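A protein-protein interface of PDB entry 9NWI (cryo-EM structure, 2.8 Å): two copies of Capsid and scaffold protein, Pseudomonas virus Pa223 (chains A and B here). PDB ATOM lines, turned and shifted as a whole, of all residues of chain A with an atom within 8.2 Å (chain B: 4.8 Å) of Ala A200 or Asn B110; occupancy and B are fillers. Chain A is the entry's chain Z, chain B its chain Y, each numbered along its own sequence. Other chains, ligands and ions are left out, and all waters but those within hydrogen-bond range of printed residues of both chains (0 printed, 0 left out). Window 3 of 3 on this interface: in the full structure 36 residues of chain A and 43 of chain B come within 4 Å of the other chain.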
ATOM      1  N   PRO A 167      12.052   5.666  24.652  1.00  0.00           N
ATOM      2  CA  PRO A 167      13.448   5.719  24.194  1.00  0.00           C
ATOM      3  C   PRO A 167      14.037   7.113  24.046  1.00  0.00           C
ATOM      4  O   PRO A 167      15.245   7.216  23.811  1.00  0.00           O
ATOM      5  CB  PRO A 167      13.342   5.050  22.821  1.00  0.00           C
ATOM      6  CG  PRO A 167      12.001   5.500  22.314  1.00  0.00           C
ATOM      7  CD  PRO A 167      11.109   5.713  23.523  1.00  0.00           C
ATOM      8  N   GLN A 168      13.238   8.168  24.160  1.00  0.00           N
ATOM      9  CA  GLN A 168      13.715   9.518  23.902  1.00  0.00           C
ATOM     10  C   GLN A 168      13.797  10.350  25.173  1.00  0.00           C
ATOM     11  O   GLN A 168      13.530  11.552  25.145  1.00  0.00           O
ATOM     12  CB  GLN A 168      12.840  10.217  22.865  1.00  0.00           C
ATOM     13  CG  GLN A 168      13.087   9.753  21.446  1.00  0.00           C
ATOM     14  CD  GLN A 168      12.044  10.264  20.481  1.00  0.00           C
ATOM     15  OE1 GLN A 168      10.959  10.678  20.887  1.00  0.00           O
ATOM     16  NE2 GLN A 168      12.363  10.235  19.194  1.00  0.00           N
ATOM     17  N   MET A 169      14.165   9.742  26.298  1.00  0.00           N
ATOM     18  CA  MET A 169      14.428  10.529  27.491  1.00  0.00           C
ATOM     19  C   MET A 169      15.563   9.920  28.297  1.00  0.00           C
ATOM     20  O   MET A 169      15.851   8.724  28.196  1.00  0.00           O
ATOM     21  CB  MET A 169      13.201  10.671  28.389  1.00  0.00           C
ATOM     22  CG  MET A 169      12.441   9.413  28.694  1.00  0.00           C
ATOM     23  SD  MET A 169      13.043   8.830  30.286  1.00  0.00           S
ATOM     24  CE  MET A 169      11.768   9.468  31.365  1.00  0.00           C
ATOM     25  N   ASN A 197      14.459  13.879  31.780  1.00  0.00           N
ATOM     26  CA  ASN A 197      14.218  14.882  30.749  1.00  0.00           C
ATOM     27  C   ASN A 197      14.156  14.207  29.390  1.00  0.00           C
ATOM     28  O   ASN A 197      14.935  13.305  29.092  1.00  0.00           O
ATOM     29  CB  ASN A 197      15.293  15.971  30.741  1.00  0.00           C
ATOM     30  CG  ASN A 197      14.936  17.122  29.827  1.00  0.00           C
ATOM     31  OD1 ASN A 197      13.773  17.310  29.475  1.00  0.00           O
ATOM     32  ND2 ASN A 197      15.937  17.894  29.426  1.00  0.00           N
ATOM     33  N   THR A 198      13.249  14.687  28.544  1.00  0.00           N
ATOM     34  CA  THR A 198      12.993  14.055  27.258  1.00  0.00           C
ATOM     35  C   THR A 198      13.501  14.937  26.128  1.00  0.00           C
ATOM     36  O   THR A 198      13.157  16.120  26.050  1.00  0.00           O
ATOM     37  CB  THR A 198      11.500  13.755  27.078  1.00  0.00           C
ATOM     38  OG1 THR A 198      11.247  13.359  25.726  1.00  0.00           O
ATOM     39  CG2 THR A 198      10.650  14.968  27.429  1.00  0.00           C
ATOM     40  N   LEU A 199      14.332  14.359  25.266  1.00  0.00           N
ATOM     41  CA  LEU A 199      14.835  15.044  24.076  1.00  0.00           C
ATOM     42  C   LEU A 199      14.005  14.658  22.855  1.00  0.00           C
ATOM     43  O   LEU A 199      14.488  14.047  21.904  1.00  0.00           O
ATOM     44  CB  LEU A 199      16.309  14.718  23.863  1.00  0.00           C
ATOM     45  CG  LEU A 199      17.243  14.953  25.048  1.00  0.00           C
ATOM     46  CD1 LEU A 199      18.653  14.521  24.699  1.00  0.00           C
ATOM     47  CD2 LEU A 199      17.215  16.412  25.459  1.00  0.00           C
ATOM     48  N   ALA A 200      12.732  15.030  22.893  1.00  0.00           N
ATOM     49  CA  ALA A 200      11.757  14.591  21.900  1.00  0.00           C
ATOM     50  C   ALA A 200      11.386  15.770  21.005  1.00  0.00           C
ATOM     51  O   ALA A 200      10.416  16.485  21.260  1.00  0.00           O
ATOM     52  CB  ALA A 200      10.531  14.000  22.578  1.00  0.00           C
ATOM     53  N   ASP A 201      12.173  15.968  19.948  1.00  0.00           N
ATOM     54  CA  ASP A 201      11.808  16.895  18.887  1.00  0.00           C
ATOM     55  C   ASP A 201      12.182  16.345  17.517  1.00  0.00           C
ATOM     56  O   ASP A 201      12.005  17.048  16.514  1.00  0.00           O
ATOM     57  CB  ASP A 201      12.459  18.264  19.103  1.00  0.00           C
ATOM     58  CG  ASP A 201      13.969  18.187  19.169  1.00  0.00           C
ATOM     59  OD1 ASP A 201      14.502  17.067  19.314  1.00  0.00           O
ATOM     60  OD2 ASP A 201      14.622  19.247  19.078  1.00  0.00           O
ATOM     61  N   THR A 202      12.695  15.120  17.448  1.00  0.00           N
ATOM     62  CA  THR A 202      13.042  14.474  16.194  1.00  0.00           C
ATOM     63  C   THR A 202      12.772  12.984  16.353  1.00  0.00           C
ATOM     64  O   THR A 202      12.811  12.451  17.464  1.00  0.00           O
ATOM     65  CB  THR A 202      14.506  14.731  15.816  1.00  0.00           C
ATOM     66  OG1 THR A 202      14.779  16.134  15.911  1.00  0.00           O
ATOM     67  CG2 THR A 202      14.784  14.285  14.391  1.00  0.00           C
ATOM     68  N   ASN A 203      12.493  12.316  15.232  1.00  0.00           N
ATOM     69  CA  ASN A 203      12.097  10.914  15.274  1.00  0.00           C
ATOM     70  C   ASN A 203      13.199   9.994  15.782  1.00  0.00           C
ATOM     71  O   ASN A 203      12.909   8.841  16.119  1.00  0.00           O
ATOM     72  CB  ASN A 203      11.648  10.461  13.885  1.00  0.00           C
ATOM     73  CG  ASN A 203      10.798   9.211  13.931  1.00  0.00           C
ATOM     74  OD1 ASN A 203      10.909   8.340  13.071  1.00  0.00           O
ATOM     75  ND2 ASN A 203       9.947   9.113  14.944  1.00  0.00           N
ATOM     76  N   GLY A 204      14.440  10.462  15.850  1.00  0.00           N
ATOM     77  CA  GLY A 204      15.526   9.621  16.304  1.00  0.00           C
ATOM     78  C   GLY A 204      15.452   9.323  17.788  1.00  0.00           C
ATOM     79  O   GLY A 204      14.673   9.904  18.543  1.00  0.00           O
ATOM     80  N   ILE A 206      18.001   8.082  21.376  1.00  0.00           N
ATOM     81  CA  ILE A 206      19.345   8.054  21.938  1.00  0.00           C
ATOM     82  C   ILE A 206      19.980   6.700  21.677  1.00  0.00           C
ATOM     83  O   ILE A 206      19.349   5.652  21.861  1.00  0.00           O
ATOM     84  CB  ILE A 206      19.334   8.378  23.441  1.00  0.00           C
ATOM     85  CG1 ILE A 206      18.697   9.742  23.738  1.00  0.00           C
ATOM     86  CG2 ILE A 206      20.738   8.318  24.008  1.00  0.00           C
ATOM     87  CD1 ILE A 206      17.201   9.768  23.778  1.00  0.00           C
ATOM     88  N   LYS A 220      21.993  10.990  19.237  1.00  0.00           N
ATOM     89  CA  LYS A 220      20.775  10.402  18.719  1.00  0.00           C
ATOM     90  C   LYS A 220      21.059   9.827  17.335  1.00  0.00           C
ATOM     91  O   LYS A 220      22.195   9.840  16.855  1.00  0.00           O
ATOM     92  CB  LYS A 220      19.655  11.442  18.691  1.00  0.00           C
ATOM     93  CG  LYS A 220      19.091  11.774  20.059  1.00  0.00           C
ATOM     94  CD  LYS A 220      17.954  12.779  19.972  1.00  0.00           C
ATOM     95  CE  LYS A 220      17.101  12.559  18.737  1.00  0.00           C
ATOM     96  NZ  LYS A 220      15.651  12.681  19.039  1.00  0.00           N
ATOM     97  N   TYR A 225      23.311  16.196  21.072  1.00  0.00           N
ATOM     98  CA  TYR A 225      23.019  17.102  22.172  1.00  0.00           C
ATOM     99  C   TYR A 225      24.149  17.065  23.192  1.00  0.00           C
ATOM    100  O   TYR A 225      24.976  16.151  23.201  1.00  0.00           O
ATOM    101  CB  TYR A 225      21.705  16.734  22.872  1.00  0.00           C
ATOM    102  CG  TYR A 225      20.469  16.959  22.042  1.00  0.00           C
ATOM    103  CD1 TYR A 225      20.087  16.048  21.071  1.00  0.00           C
ATOM    104  CD2 TYR A 225      19.677  18.079  22.236  1.00  0.00           C
ATOM    105  CE1 TYR A 225      18.956  16.249  20.312  1.00  0.00           C
ATOM    106  CE2 TYR A 225      18.544  18.289  21.482  1.00  0.00           C
ATOM    107  CZ  TYR A 225      18.187  17.370  20.521  1.00  0.00           C
ATOM    108  OH  TYR A 225      17.057  17.574  19.767  1.00  0.00           O
ATOM    109  N   SER B 108       7.746  15.398  14.159  1.00  0.00           N
ATOM    110  CA  SER B 108       7.589  14.529  15.312  1.00  0.00           C
ATOM    111  C   SER B 108       7.738  15.341  16.591  1.00  0.00           C
ATOM    112  O   SER B 108       8.533  16.282  16.659  1.00  0.00           O
ATOM    113  CB  SER B 108       8.612  13.392  15.296  1.00  0.00           C
ATOM    114  OG  SER B 108       9.863  13.834  15.787  1.00  0.00           O
ATOM    115  N   PHE B 109       6.962  14.967  17.603  1.00  0.00           N
ATOM    116  CA  PHE B 109       6.992  15.657  18.889  1.00  0.00           C
ATOM    117  C   PHE B 109       6.512  14.692  19.956  1.00  0.00           C
ATOM    118  O   PHE B 109       5.369  14.227  19.896  1.00  0.00           O
ATOM    119  CB  PHE B 109       6.116  16.903  18.857  1.00  0.00           C
ATOM    120  CG  PHE B 109       5.978  17.576  20.187  1.00  0.00           C
ATOM    121  CD1 PHE B 109       7.060  18.202  20.775  1.00  0.00           C
ATOM    122  CD2 PHE B 109       4.769  17.573  20.854  1.00  0.00           C
ATOM    123  CE1 PHE B 109       6.936  18.822  22.000  1.00  0.00           C
ATOM    124  CE2 PHE B 109       4.640  18.192  22.079  1.00  0.00           C
ATOM    125  CZ  PHE B 109       5.724  18.815  22.653  1.00  0.00           C
ATOM    126  N   ASN B 110       7.379  14.389  20.923  1.00  0.00           N
ATOM    127  CA  ASN B 110       7.049  13.495  22.032  1.00  0.00           C
ATOM    128  C   ASN B 110       6.596  12.125  21.542  1.00  0.00           C
ATOM    129  O   ASN B 110       5.721  11.496  22.142  1.00  0.00           O
ATOM    130  CB  ASN B 110       5.987  14.114  22.943  1.00  0.00           C
ATOM    131  CG  ASN B 110       6.589  14.934  24.061  1.00  0.00           C
ATOM    132  OD1 ASN B 110       7.790  14.867  24.315  1.00  0.00           O
ATOM    133  ND2 ASN B 110       5.756  15.718  24.732  1.00  0.00           N
ATOM    134  N   GLY B 111       7.181  11.652  20.445  1.00  0.00           N
ATOM    135  CA  GLY B 111       6.808  10.375  19.876  1.00  0.00           C
ATOM    136  C   GLY B 111       5.532  10.384  19.068  1.00  0.00           C
ATOM    137  O   GLY B 111       5.113   9.322  18.593  1.00  0.00           O
ATOM    138  N   VAL B 112       4.903  11.542  18.891  1.00  0.00           N
ATOM    139  CA  VAL B 112       3.655  11.672  18.150  1.00  0.00           C
ATOM    140  C   VAL B 112       3.957  12.396  16.848  1.00  0.00           C
ATOM    141  O   VAL B 112       4.633  13.431  16.852  1.00  0.00           O
ATOM    142  CB  VAL B 112       2.597  12.429  18.969  1.00  0.00           C
ATOM    143  CG1 VAL B 112       1.410  12.797  18.098  1.00  0.00           C
ATOM    144  CG2 VAL B 112       2.159  11.597  20.158  1.00  0.00           C
ATOM    145  N   LYS B 151      12.352  22.166  20.978  1.00  0.00           N
ATOM    146  CA  LYS B 151      12.603  21.771  22.367  1.00  0.00           C
ATOM    147  C   LYS B 151      11.358  21.058  22.878  1.00  0.00           C
ATOM    148  O   LYS B 151      11.022  19.987  22.342  1.00  0.00           O
ATOM    149  CB  LYS B 151      13.045  22.998  23.166  1.00  0.00           C
ATOM    150  CG  LYS B 151      14.417  23.515  22.789  1.00  0.00           C
ATOM    151  CD  LYS B 151      15.438  23.192  23.862  1.00  0.00           C
ATOM    152  CE  LYS B 151      16.742  23.929  23.622  1.00  0.00           C
ATOM    153  NZ  LYS B 151      17.304  23.627  22.279  1.00  0.00           N
ATOM    154  N   ALA B 176       4.528  21.156  28.600  1.00  0.00           N
ATOM    155  CA  ALA B 176       3.894  19.839  28.650  1.00  0.00           C
ATOM    156  C   ALA B 176       4.918  18.720  28.426  1.00  0.00           C
ATOM    157  O   ALA B 176       4.883  17.984  27.442  1.00  0.00           O
ATOM    158  CB  ALA B 176       2.752  19.750  27.636  1.00  0.00           C
ATOM    159  N   GLY B 179       6.181  13.586  27.855  1.00  0.00           N
ATOM    160  CA  GLY B 179       5.430  13.016  26.759  1.00  0.00           C
ATOM    161  C   GLY B 179       4.083  13.684  26.552  1.00  0.00           C
ATOM    162  O   GLY B 179       3.722  14.669  27.201  1.00  0.00           O
ATOM    163  N   GLY B 180       3.326  13.117  25.618  1.00  0.00           N
ATOM    164  CA  GLY B 180       2.008  13.627  25.308  1.00  0.00           C
ATOM    165  C   GLY B 180       2.057  14.879  24.449  1.00  0.00           C
ATOM    166  O   GLY B 180       3.105  15.321  23.978  1.00  0.00           O
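The side-chain hydroxyl (OG) of Ser B108 lies within hydrogen-bond range of the backbone NH (N) of Asn A203 (3.1 Å).
OD1 of Asp A201 sits at hydrogen-bond distance from OH of Tyr A225 (2.6 Å). The backbone carbonyl oxygen (O) of Gln A168 lies within hydrogen-bond range of the backbone NH (N) of Leu A199, 2.9 Å away. NZ of Lys A220 lies within hydrogen-bond range of O of Thr A202 (3.3 Å). The side-chain amide nitrogen (NE2) of Gln A168 lies within hydrogen-bond range of the backbone carbonyl oxygen (O) of Thr A202. The backbone carbonyl oxygen of Asn A203 lies within hydrogen-bond range of the side-chain amide nitrogen of Gln A168. The side-chain amide nitrogen (ND2) of Asn B110 lies within hydrogen-bond range of the backbone carbonyl oxygen (O) of Gly B180 (2.8 Å).
Gln A168 touches Gly B111. Ala A200 touches Phe B109. CB of Ala A200 touches OD1 of Asn B110, 3.4 Å away. Ala A200 touches Lys B151 (O to O, 3.7 Å). Ser B108 touches Asp A201. Asp A201 touches Lys B151 (CB to O, 3.9 Å). C of Thr A202 touches OG of Ser B108, at 3.1 Å.
Ala A200 touches just these residues of chain B: Phe B109, Asn B110 and Lys B151. Of the printed residues of chain B, Asp A201 touches Ser B108 and Lys B151. Of the printed residues of chain A, Gly B111 touches Gln A168. Tyr A225 touches none of the printed residues of chain B. Pro A167 touches none of the printed residues of chain B. The nearest residue of chain A that does not touch Asn B110 is Thr A198 (4.03 Å).
Along chain B the printed residues that touch a printed residue of chain A span positions 108 to 151. Of the 14 printed residues of chain A, 5 touch a printed residue of chain B. Hydrophobic or aromatic side chains of chain A that line the printed part of chain B: Ala A200. Among the printed residues, 8 pairs touch across the chains. Among the printed residues, no Asp or Glu carboxylate lies within 4 Å of a Lys or Arg side-chain nitrogen of the other chain.
No position is printed for both chains. Of the 8 pairs that touch across the chains among the printed residues, none has its exchanged pair printed and touching as well.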
